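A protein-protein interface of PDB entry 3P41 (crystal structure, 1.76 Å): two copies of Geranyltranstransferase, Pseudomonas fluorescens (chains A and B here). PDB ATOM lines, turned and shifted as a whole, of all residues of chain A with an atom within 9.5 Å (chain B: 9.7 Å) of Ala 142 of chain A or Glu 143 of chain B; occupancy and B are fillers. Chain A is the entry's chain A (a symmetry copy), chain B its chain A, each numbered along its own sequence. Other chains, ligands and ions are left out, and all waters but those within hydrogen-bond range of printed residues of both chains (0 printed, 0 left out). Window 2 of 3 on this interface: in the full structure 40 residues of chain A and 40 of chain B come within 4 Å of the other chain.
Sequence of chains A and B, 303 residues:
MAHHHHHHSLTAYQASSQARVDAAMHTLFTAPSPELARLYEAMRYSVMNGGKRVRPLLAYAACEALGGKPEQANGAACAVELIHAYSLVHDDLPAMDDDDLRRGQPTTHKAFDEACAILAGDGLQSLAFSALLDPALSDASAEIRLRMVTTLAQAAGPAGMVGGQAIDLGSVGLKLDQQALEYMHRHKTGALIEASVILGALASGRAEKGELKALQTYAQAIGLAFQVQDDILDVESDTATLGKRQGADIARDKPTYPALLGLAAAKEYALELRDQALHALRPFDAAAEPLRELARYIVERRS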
ATOM      1  N   LEU A 132       9.594  36.595 -18.098  1.00  0.00           N
ATOM      2  CA  LEU A 132       8.724  35.428 -18.076  1.00  0.00           C
ATOM      3  C   LEU A 132       9.563  34.158 -18.137  1.00  0.00           C
ATOM      4  O   LEU A 132       9.162  33.102 -17.685  1.00  0.00           O
ATOM      5  CB  LEU A 132       7.803  35.483 -19.291  1.00  0.00           C
ATOM      6  CG  LEU A 132       6.455  34.758 -19.292  1.00  0.00           C
ATOM      7  CD1 LEU A 132       5.589  35.124 -18.091  1.00  0.00           C
ATOM      8  CD2 LEU A 132       5.745  35.057 -20.606  1.00  0.00           C
ATOM      9  N   LEU A 133      10.753  34.276 -18.708  1.00  0.00           N
ATOM     10  CA  LEU A 133      11.601  33.130 -18.941  1.00  0.00           C
ATOM     11  C   LEU A 133      12.823  33.116 -18.024  1.00  0.00           C
ATOM     12  O   LEU A 133      13.649  32.227 -18.116  1.00  0.00           O
ATOM     13  CB  LEU A 133      12.085  33.128 -20.394  1.00  0.00           C
ATOM     14  CG  LEU A 133      11.020  32.923 -21.484  1.00  0.00           C
ATOM     15  CD1 LEU A 133      11.679  32.360 -22.738  1.00  0.00           C
ATOM     16  CD2 LEU A 133       9.879  32.009 -21.030  1.00  0.00           C
ATOM     17  N   ASP A 139      10.243  28.550 -11.568  1.00  0.00           N
ATOM     18  CA  ASP A 139      10.870  27.236 -11.736  1.00  0.00           C
ATOM     19  C   ASP A 139      10.096  26.407 -12.749  1.00  0.00           C
ATOM     20  O   ASP A 139      10.391  25.231 -12.927  1.00  0.00           O
ATOM     21  CB  ASP A 139      10.924  26.426 -10.424  1.00  0.00           C
ATOM     22  CG  ASP A 139      10.788  27.289  -9.167  1.00  0.00           C
ATOM     23  OD1 ASP A 139       9.672  27.798  -8.893  1.00  0.00           O
ATOM     24  OD2 ASP A 139      11.792  27.410  -8.421  1.00  0.00           O
ATOM     25  N   ALA A 140       9.088  26.993 -13.395  1.00  0.00           N
ATOM     26  CA  ALA A 140       8.208  26.225 -14.298  1.00  0.00           C
ATOM     27  C   ALA A 140       8.922  25.381 -15.371  1.00  0.00           C
ATOM     28  O   ALA A 140      10.053  25.672 -15.752  1.00  0.00           O
ATOM     29  CB  ALA A 140       7.162  27.139 -14.939  1.00  0.00           C
ATOM     30  N   SER A 141       8.206  24.321 -15.768  1.00  0.00           N
ATOM     31  CA  SER A 141       8.652  23.280 -16.708  1.00  0.00           C
ATOM     32  C   SER A 141       8.468  23.742 -18.139  1.00  0.00           C
ATOM     33  O   SER A 141       7.716  24.679 -18.399  1.00  0.00           O
ATOM     34  CB  SER A 141       7.871  21.976 -16.491  1.00  0.00           C
ATOM     35  OG  SER A 141       6.642  21.952 -17.214  1.00  0.00           O
ATOM     36  N   ALA A 142       9.144  23.064 -19.062  1.00  0.00           N
ATOM     37  CA  ALA A 142       9.300  23.546 -20.445  1.00  0.00           C
ATOM     38  C   ALA A 142       7.999  23.867 -21.183  1.00  0.00           C
ATOM     39  O   ALA A 142       7.852  24.959 -21.725  1.00  0.00           O
ATOM     40  CB  ALA A 142      10.168  22.562 -21.268  1.00  0.00           C
ATOM     41  N   GLU A 143       7.064  22.916 -21.214  1.00  0.00           N
ATOM     42  CA  GLU A 143       5.790  23.095 -21.938  1.00  0.00           C
ATOM     43  C   GLU A 143       4.828  24.094 -21.266  1.00  0.00           C
ATOM     44  O   GLU A 143       4.094  24.811 -21.943  1.00  0.00           O
ATOM     45  CB  GLU A 143       5.087  21.748 -22.136  1.00  0.00           C
ATOM     46  CG  GLU A 143       5.935  20.690 -22.824  1.00  0.00           C
ATOM     47  CD  GLU A 143       6.064  20.926 -24.307  1.00  0.00           C
ATOM     48  OE1 GLU A 143       5.214  21.662 -24.870  1.00  0.00           O
ATOM     49  OE2 GLU A 143       7.014  20.378 -24.906  1.00  0.00           O
ATOM     50  N   ILE A 144       4.824  24.130 -19.938  1.00  0.00           N
ATOM     51  CA  ILE A 144       4.009  25.117 -19.210  1.00  0.00           C
ATOM     52  C   ILE A 144       4.437  26.524 -19.609  1.00  0.00           C
ATOM     53  O   ILE A 144       3.615  27.401 -19.865  1.00  0.00           O
ATOM     54  CB  ILE A 144       4.167  24.968 -17.684  1.00  0.00           C
ATOM     55  CG1 ILE A 144       3.312  23.808 -17.170  1.00  0.00           C
ATOM     56  CG2 ILE A 144       3.820  26.270 -16.969  1.00  0.00           C
ATOM     57  CD1 ILE A 144       3.182  23.767 -15.660  1.00  0.00           C
ATOM     58  N   ARG A 145       5.744  26.727 -19.672  1.00  0.00           N
ATOM     59  CA  ARG A 145       6.308  28.032 -19.986  1.00  0.00           C
ATOM     60  C   ARG A 145       6.138  28.410 -21.454  1.00  0.00           C
ATOM     61  O   ARG A 145       6.160  29.588 -21.804  1.00  0.00           O
ATOM     62  CB  ARG A 145       7.782  28.056 -19.595  1.00  0.00           C
ATOM     63  CG  ARG A 145       8.016  28.082 -18.090  1.00  0.00           C
ATOM     64  CD  ARG A 145       9.509  28.103 -17.764  1.00  0.00           C
ATOM     65  NE  ARG A 145      10.233  27.101 -18.532  1.00  0.00           N
ATOM     66  CZ  ARG A 145      11.544  26.901 -18.456  1.00  0.00           C
ATOM     67  NH1 ARG A 145      12.282  27.638 -17.640  1.00  0.00           N
ATOM     68  NH2 ARG A 145      12.114  25.963 -19.195  1.00  0.00           N
ATOM     69  N   LEU A 146       5.979  27.409 -22.315  1.00  0.00           N
ATOM     70  CA  LEU A 146       5.596  27.649 -23.702  1.00  0.00           C
ATOM     71  C   LEU A 146       4.154  28.144 -23.728  1.00  0.00           C
ATOM     72  O   LEU A 146       3.821  29.136 -24.368  1.00  0.00           O
ATOM     73  CB  LEU A 146       5.747  26.354 -24.505  1.00  0.00           C
ATOM     74  CG  LEU A 146       5.241  26.241 -25.950  1.00  0.00           C
ATOM     75  CD1 LEU A 146       5.695  27.402 -26.822  1.00  0.00           C
ATOM     76  CD2 LEU A 146       5.710  24.913 -26.549  1.00  0.00           C
ATOM     77  N   ARG A 147       3.297  27.455 -22.997  1.00  0.00           N
ATOM     78  CA  ARG A 147       1.922  27.896 -22.846  1.00  0.00           C
ATOM     79  C   ARG A 147       1.893  29.352 -22.369  1.00  0.00           C
ATOM     80  O   ARG A 147       1.351  30.217 -23.050  1.00  0.00           O
ATOM     81  CB  ARG A 147       1.177  26.958 -21.893  1.00  0.00           C
ATOM     82  CG  ARG A 147       1.070  25.520 -22.421  1.00  0.00           C
ATOM     83  CD  ARG A 147       0.706  24.507 -21.340  1.00  0.00           C
ATOM     84  NE  ARG A 147      -0.725  24.478 -21.034  1.00  0.00           N
ATOM     85  CZ  ARG A 147      -1.268  23.756 -20.055  1.00  0.00           C
ATOM     86  NH1 ARG A 147      -0.499  23.003 -19.279  1.00  0.00           N
ATOM     87  NH2 ARG A 147      -2.580  23.787 -19.846  1.00  0.00           N
ATOM     88  N   MET A 148       2.496  29.622 -21.215  1.00  0.00           N
ATOM     89  CA  MET A 148       2.641  30.991 -20.739  1.00  0.00           C
ATOM     90  C   MET A 148       3.181  31.980 -21.810  1.00  0.00           C
ATOM     91  O   MET A 148       2.545  32.984 -22.096  1.00  0.00           O
ATOM     92  CB  MET A 148       3.501  31.049 -19.464  1.00  0.00           C
ATOM     93  CG  MET A 148       3.304  29.913 -18.519  1.00  0.00           C
ATOM     94  SD  MET A 148       4.214  30.179 -16.823  1.00  0.00           S
ATOM     95  CE  MET A 148       6.053  30.331 -17.433  1.00  0.00           C
ATOM     96  N   VAL A 149       4.344  31.741 -22.413  1.00  0.00           N
ATOM     97  CA  VAL A 149       4.865  32.755 -23.352  1.00  0.00           C
ATOM     98  C   VAL A 149       3.967  33.161 -24.517  1.00  0.00           C
ATOM     99  O   VAL A 149       3.826  34.373 -24.821  1.00  0.00           O
ATOM    100  CB  VAL A 149       6.236  32.369 -23.967  1.00  0.00           C
ATOM    101  CG1 VAL A 149       6.425  33.138 -25.268  1.00  0.00           C
ATOM    102  CG2 VAL A 149       7.293  32.731 -23.018  1.00  0.00           C
ATOM    103  N   THR A 150       3.405  32.128 -25.160  1.00  0.00           N
ATOM    104  CA  THR A 150       2.404  32.106 -26.211  1.00  0.00           C
ATOM    105  C   THR A 150       1.203  32.913 -25.778  1.00  0.00           C
ATOM    106  O   THR A 150       0.702  33.755 -26.524  1.00  0.00           O
ATOM    107  CB  THR A 150       1.939  30.669 -26.490  1.00  0.00           C
ATOM    108  OG1 THR A 150       3.025  29.944 -27.068  1.00  0.00           O
ATOM    109  CG2 THR A 150       0.759  30.661 -27.457  1.00  0.00           C
ATOM    110  N   LEU A 202      -0.871  28.907 -14.448  1.00  0.00           N
ATOM    111  CA  LEU A 202       0.060  28.038 -15.122  1.00  0.00           C
ATOM    112  C   LEU A 202       1.324  27.912 -14.292  1.00  0.00           C
ATOM    113  O   LEU A 202       1.909  26.823 -14.190  1.00  0.00           O
ATOM    114  CB  LEU A 202       0.375  28.596 -16.507  1.00  0.00           C
ATOM    115  CG  LEU A 202      -0.582  28.322 -17.647  1.00  0.00           C
ATOM    116  CD1 LEU A 202      -0.039  28.977 -18.904  1.00  0.00           C
ATOM    117  CD2 LEU A 202      -0.803  26.802 -17.834  1.00  0.00           C
ATOM    118  N   LEU B 133       7.130  30.921 -31.782  1.00  0.00           N
ATOM    119  CA  LEU B 133       6.582  29.803 -31.052  1.00  0.00           C
ATOM    120  C   LEU B 133       5.455  29.108 -31.812  1.00  0.00           C
ATOM    121  O   LEU B 133       4.871  28.162 -31.317  1.00  0.00           O
ATOM    122  CB  LEU B 133       6.036  30.281 -29.702  1.00  0.00           C
ATOM    123  CG  LEU B 133       7.058  30.815 -28.685  1.00  0.00           C
ATOM    124  CD1 LEU B 133       6.491  30.675 -27.277  1.00  0.00           C
ATOM    125  CD2 LEU B 133       8.412  30.110 -28.783  1.00  0.00           C
ATOM    126  N   ASP B 139       9.436  23.084 -35.940  1.00  0.00           N
ATOM    127  CA  ASP B 139       9.147  21.847 -35.211  1.00  0.00           C
ATOM    128  C   ASP B 139      10.047  21.730 -33.989  1.00  0.00           C
ATOM    129  O   ASP B 139      10.043  20.700 -33.327  1.00  0.00           O
ATOM    130  CB  ASP B 139       9.368  20.582 -36.067  1.00  0.00           C
ATOM    131  CG  ASP B 139       9.353  20.853 -37.574  1.00  0.00           C
ATOM    132  OD1 ASP B 139      10.321  21.464 -38.094  1.00  0.00           O
ATOM    133  OD2 ASP B 139       8.393  20.402 -38.246  1.00  0.00           O
ATOM    134  N   ALA B 140      10.840  22.761 -33.699  1.00  0.00           N
ATOM    135  CA  ALA B 140      11.833  22.678 -32.610  1.00  0.00           C
ATOM    136  C   ALA B 140      11.294  22.204 -31.247  1.00  0.00           C
ATOM    137  O   ALA B 140      10.106  22.336 -30.959  1.00  0.00           O
ATOM    138  CB  ALA B 140      12.582  24.004 -32.461  1.00  0.00           C
ATOM    139  N   SER B 141      12.227  21.617 -30.487  1.00  0.00           N
ATOM    140  CA  SER B 141      12.003  20.982 -29.180  1.00  0.00           C
ATOM    141  C   SER B 141      11.989  22.022 -28.078  1.00  0.00           C
ATOM    142  O   SER B 141      12.469  23.138 -28.269  1.00  0.00           O
ATOM    143  CB  SER B 141      13.094  19.944 -28.881  1.00  0.00           C
ATOM    144  OG  SER B 141      14.249  20.526 -28.281  1.00  0.00           O
ATOM    145  N   ALA B 142      11.453  21.641 -26.922  1.00  0.00           N
ATOM    146  CA  ALA B 142      11.106  22.595 -25.856  1.00  0.00           C
ATOM    147  C   ALA B 142      12.245  23.504 -25.388  1.00  0.00           C
ATOM    148  O   ALA B 142      12.086  24.722 -25.353  1.00  0.00           O
ATOM    149  CB  ALA B 142      10.467  21.857 -24.654  1.00  0.00           C
ATOM    150  N   GLU B 143      13.383  22.916 -25.018  1.00  0.00           N
ATOM    151  CA  GLU B 143      14.531  23.689 -24.504  1.00  0.00           C
ATOM    152  C   GLU B 143      15.250  24.525 -25.579  1.00  0.00           C
ATOM    153  O   GLU B 143      15.746  25.616 -25.299  1.00  0.00           O
ATOM    154  CB  GLU B 143      15.535  22.764 -23.806  1.00  0.00           C
ATOM    155  CG  GLU B 143      14.941  21.910 -22.698  1.00  0.00           C
ATOM    156  CD  GLU B 143      14.675  22.697 -21.439  1.00  0.00           C
ATOM    157  OE1 GLU B 143      15.285  23.784 -21.277  1.00  0.00           O
ATOM    158  OE2 GLU B 143      13.861  22.228 -20.616  1.00  0.00           O
ATOM    159  N   ILE B 144      15.318  24.011 -26.801  1.00  0.00           N
ATOM    160  CA  ILE B 144      15.900  24.777 -27.915  1.00  0.00           C
ATOM    161  C   ILE B 144      15.116  26.069 -28.109  1.00  0.00           C
ATOM    162  O   ILE B 144      15.678  27.146 -28.283  1.00  0.00           O
ATOM    163  CB  ILE B 144      15.868  23.978 -29.233  1.00  0.00           C
ATOM    164  CG1 ILE B 144      17.012  22.962 -29.268  1.00  0.00           C
ATOM    165  CG2 ILE B 144      15.920  24.910 -30.439  1.00  0.00           C
ATOM    166  CD1 ILE B 144      17.230  22.335 -30.631  1.00  0.00           C
ATOM    167  N   ARG B 145      13.797  25.949 -28.065  1.00  0.00           N
ATOM    168  CA  ARG B 145      12.911  27.081 -28.287  1.00  0.00           C
ATOM    169  C   ARG B 145      12.902  28.060 -27.117  1.00  0.00           C
ATOM    170  O   ARG B 145      12.568  29.232 -27.284  1.00  0.00           O
ATOM    171  CB  ARG B 145      11.501  26.574 -28.571  1.00  0.00           C
ATOM    172  CG  ARG B 145      11.350  25.919 -29.938  1.00  0.00           C
ATOM    173  CD  ARG B 145       9.918  25.431 -30.162  1.00  0.00           C
ATOM    174  NE  ARG B 145       9.426  24.690 -29.010  1.00  0.00           N
ATOM    175  CZ  ARG B 145       8.212  24.158 -28.926  1.00  0.00           C
ATOM    176  NH1 ARG B 145       7.359  24.284 -29.931  1.00  0.00           N
ATOM    177  NH2 ARG B 145       7.853  23.499 -27.835  1.00  0.00           N
ATOM    178  N   LEU B 146      13.256  27.578 -25.930  1.00  0.00           N
ATOM    179  CA  LEU B 146      13.492  28.455 -24.789  1.00  0.00           C
ATOM    180  C   LEU B 146      14.762  29.258 -25.048  1.00  0.00           C
ATOM    181  O   LEU B 146      14.803  30.474 -24.893  1.00  0.00           O
ATOM    182  CB  LEU B 146      13.624  27.614 -23.516  1.00  0.00           C
ATOM    183  CG  LEU B 146      14.062  28.237 -22.183  1.00  0.00           C
ATOM    184  CD1 LEU B 146      13.286  29.501 -21.845  1.00  0.00           C
ATOM    185  CD2 LEU B 146      13.905  27.203 -21.065  1.00  0.00           C
ATOM    186  N   ARG B 147      15.801  28.565 -25.476  1.00  0.00           N
ATOM    187  CA  ARG B 147      17.030  29.231 -25.870  1.00  0.00           C
ATOM    188  C   ARG B 147      16.723  30.318 -26.905  1.00  0.00           C
ATOM    189  O   ARG B 147      16.995  31.492 -26.672  1.00  0.00           O
ATOM    190  CB  ARG B 147      18.036  28.201 -26.390  1.00  0.00           C
ATOM    191  CG  ARG B 147      18.468  27.185 -25.322  1.00  0.00           C
ATOM    192  CD  ARG B 147      19.131  25.941 -25.907  1.00  0.00           C
ATOM    193  NE  ARG B 147      20.538  26.145 -26.251  1.00  0.00           N
ATOM    194  CZ  ARG B 147      21.296  25.243 -26.873  1.00  0.00           C
ATOM    195  NH1 ARG B 147      20.782  24.073 -27.226  1.00  0.00           N
ATOM    196  NH2 ARG B 147      22.569  25.510 -27.148  1.00  0.00           N
ATOM    197  N   MET B 148      16.135  29.928 -28.034  1.00  0.00           N
ATOM    198  CA  MET B 148      15.681  30.896 -29.023  1.00  0.00           C
ATOM    199  C   MET B 148      14.854  32.070 -28.428  1.00  0.00           C
ATOM    200  O   MET B 148      15.205  33.226 -28.617  1.00  0.00           O
ATOM    201  CB  MET B 148      14.904  30.207 -30.159  1.00  0.00           C
ATOM    202  CG  MET B 148      15.429  28.870 -30.561  1.00  0.00           C
ATOM    203  SD  MET B 148      14.576  28.178 -32.163  1.00  0.00           S
ATOM    204  CE  MET B 148      12.726  28.106 -31.571  1.00  0.00           C
ATOM    205  N   VAL B 149      13.756  31.821 -27.718  1.00  0.00           N
ATOM    206  CA  VAL B 149      12.950  32.967 -27.253  1.00  0.00           C
ATOM    207  C   VAL B 149      13.653  34.027 -26.411  1.00  0.00           C
ATOM    208  O   VAL B 149      13.472  35.250 -26.642  1.00  0.00           O
ATOM    209  CB  VAL B 149      11.686  32.542 -26.460  1.00  0.00           C
ATOM    210  CG1 VAL B 149      11.241  33.706 -25.584  1.00  0.00           C
ATOM    211  CG2 VAL B 149      10.625  32.205 -27.415  1.00  0.00           C
ATOM    212  N   THR B 150      14.418  33.526 -25.431  1.00  0.00           N
ATOM    213  CA  THR B 150      15.335  34.190 -24.520  1.00  0.00           C
ATOM    214  C   THR B 150      16.319  35.016 -25.312  1.00  0.00           C
ATOM    215  O   THR B 150      16.554  36.186 -25.009  1.00  0.00           O
ATOM    216  CB  THR B 150      16.126  33.160 -23.699  1.00  0.00           C
ATOM    217  OG1 THR B 150      15.224  32.494 -22.816  1.00  0.00           O
ATOM    218  CG2 THR B 150      17.217  33.846 -22.881  1.00  0.00           C
ATOM    219  N   THR B 151      16.903  34.386 -26.321  1.00  0.00           N
ATOM    220  CA  THR B 151      17.849  35.072 -27.191  1.00  0.00           C
ATOM    221  C   THR B 151      17.276  36.284 -27.900  1.00  0.00           C
ATOM    222  O   THR B 151      17.885  37.363 -27.918  1.00  0.00           O
ATOM    223  CB  THR B 151      18.467  34.080 -28.190  1.00  0.00           C
ATOM    224  OG1 THR B 151      19.055  33.000 -27.451  1.00  0.00           O
ATOM    225  CG2 THR B 151      19.531  34.753 -29.041  1.00  0.00           C
ATOM    226  N   LEU B 202      19.939  27.346 -34.076  1.00  0.00           N
ATOM    227  CA  LEU B 202      19.218  26.631 -33.054  1.00  0.00           C
ATOM    228  C   LEU B 202      18.072  25.865 -33.687  1.00  0.00           C
ATOM    229  O   LEU B 202      17.782  24.723 -33.299  1.00  0.00           O
ATOM    230  CB  LEU B 202      18.699  27.613 -32.007  1.00  0.00           C
ATOM    231  CG  LEU B 202      19.630  28.081 -30.909  1.00  0.00           C
ATOM    232  CD1 LEU B 202      18.874  29.040 -30.007  1.00  0.00           C
ATOM    233  CD2 LEU B 202      20.211  26.881 -30.124  1.00  0.00           C
ATOM    234  N   ALA B 203      17.429  26.502 -34.655  1.00  0.00           N
ATOM    235  CA  ALA B 203      16.263  25.947 -35.339  1.00  0.00           C
ATOM    236  C   ALA B 203      16.575  24.605 -36.059  1.00  0.00           C
ATOM    237  O   ALA B 203      15.695  23.774 -36.267  1.00  0.00           O
ATOM    238  CB  ALA B 203      15.743  26.967 -36.306  1.00  0.00           C
ATOM    239  N   GLY B 205      18.107  22.107 -34.853  1.00  0.00           N
ATOM    240  CA  GLY B 205      18.117  21.026 -33.871  1.00  0.00           C
ATOM    241  C   GLY B 205      19.457  20.355 -33.720  1.00  0.00           C
ATOM    242  O   GLY B 205      19.595  19.435 -32.941  1.00  0.00           O
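Leu 133 of chain A touches Leu 146 of chain B, and with the chains exchanged Leu 146 of chain A touches Leu 133 of chain B.
Leu 133 of chain A touches Val 149 of chain B, and with the chains exchanged Val 149 of chain A touches Leu 133 of chain B.
Leu 133 of chain A touches Thr 150 of chain B, and with the chains exchanged Thr 150 of chain A touches Leu 133 of chain B.
Ala 142 of chain A touches Glu 143 of chain B, and with the chains exchanged Glu 143 of chain A touches Ala 142 of chain B.
Of the 11 pairs that touch across the chains among the printed residues, 11 have their exchanged pair printed and touching as well.
Leu 146 of chain B touches Leu 133 of chain A.
CG1 of Val 149 of chain B touches CD1 of Leu 133 of chain A (3.2 Å).
Thr 150 of chain B touches Leu 133 of chain A (OG1 to CD1, 3.5 Å).
Ala 142 of chain A touches Ala 142 of chain B (CB to CB, 3.5 Å).
Glu 143 of chain A touches Ala 142 of chain B.
NH2 of Arg 145 of chain A touches CD2 of Leu 146 of chain B (2.9 Å).
Leu 133 of chain B touches Leu 146 of chain A (CD1 to CD1, 3.4 Å).
Arg 145 of chain B touches Leu 146 of chain A (NH2 to CD2, 2.9 Å).
Leu 133 of chain B touches Val 149 of chain A (CD1 to CG1, 3.2 Å).
Leu 133 of chain B touches Thr 150 of chain A.
Printed residues of chain B within 4 Å of Ala 142 of chain A: Ala 142 and Glu 143.
Of the printed residues of chain A, Glu 143 of chain B touches Ala 142 (3.8 Å).
Printed residues of chain A within 4 Å of Ala 142 of chain B: Ala 142 and Glu 143.
Of the printed residues of chain B, Glu 143 of chain A touches Ala 142 (3.8 Å).
Of the printed residues of chain B, Thr 150 of chain A touches Leu 133 (3.5 Å).
The nearest printed residue of chain B that does not touch Ala 142 of chain A is Leu 146 of chain B (5.9 Å).
The nearest printed residue of chain A that does not touch Leu 146 of chain B is Ala 142 of chain A (5.9 Å).
O of Leu 146 of chain A lies within hydrogen-bond range of OG1 of Thr 150 of chain A (2.9 Å).
The backbone carbonyl oxygen (O) of Ala 140 of chain B is in hydrogen-bond range of the guanidinium group (NE) of Arg 145 of chain B (3.1 Å).
The side-chain hydroxyl (OG1) of Thr 150 of chain B lies within hydrogen-bond range of the backbone carbonyl oxygen (O) of Leu 146 of chain B, 2.9 Å away.
The backbone carbonyl oxygen of Ala 140 of chain A lies within hydrogen-bond range of the guanidinium group of Arg 145 of chain A, 3.1 Å away.
O of Ser 141 of chain B lies close to NE of Arg 145 of chain B (3.5 Å).
NE of Arg 145 of chain A sits close to O of Ser 141 of chain A, 3.5 Å away.
Printed residues of chain B that touch a printed residue of chain A: Leu 133, Ala 142, Glu 143, Arg 145, Leu 146, Val 149 and Thr 150.
Of the 15 printed residues of chain A, 7 touch a printed residue of chain B.
Printed residues of chain A that touch a printed residue of chain B: Leu 133, Ala 142, Glu 143, Arg 145, Leu 146, Val 149 and Thr 150.
Hydrophobic or aromatic side chains of chain A that line the printed part of chain B: Leu 133, Ala 142, Leu 146 and Val 149.
Among the printed residues, 11 pairs touch across the chains.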
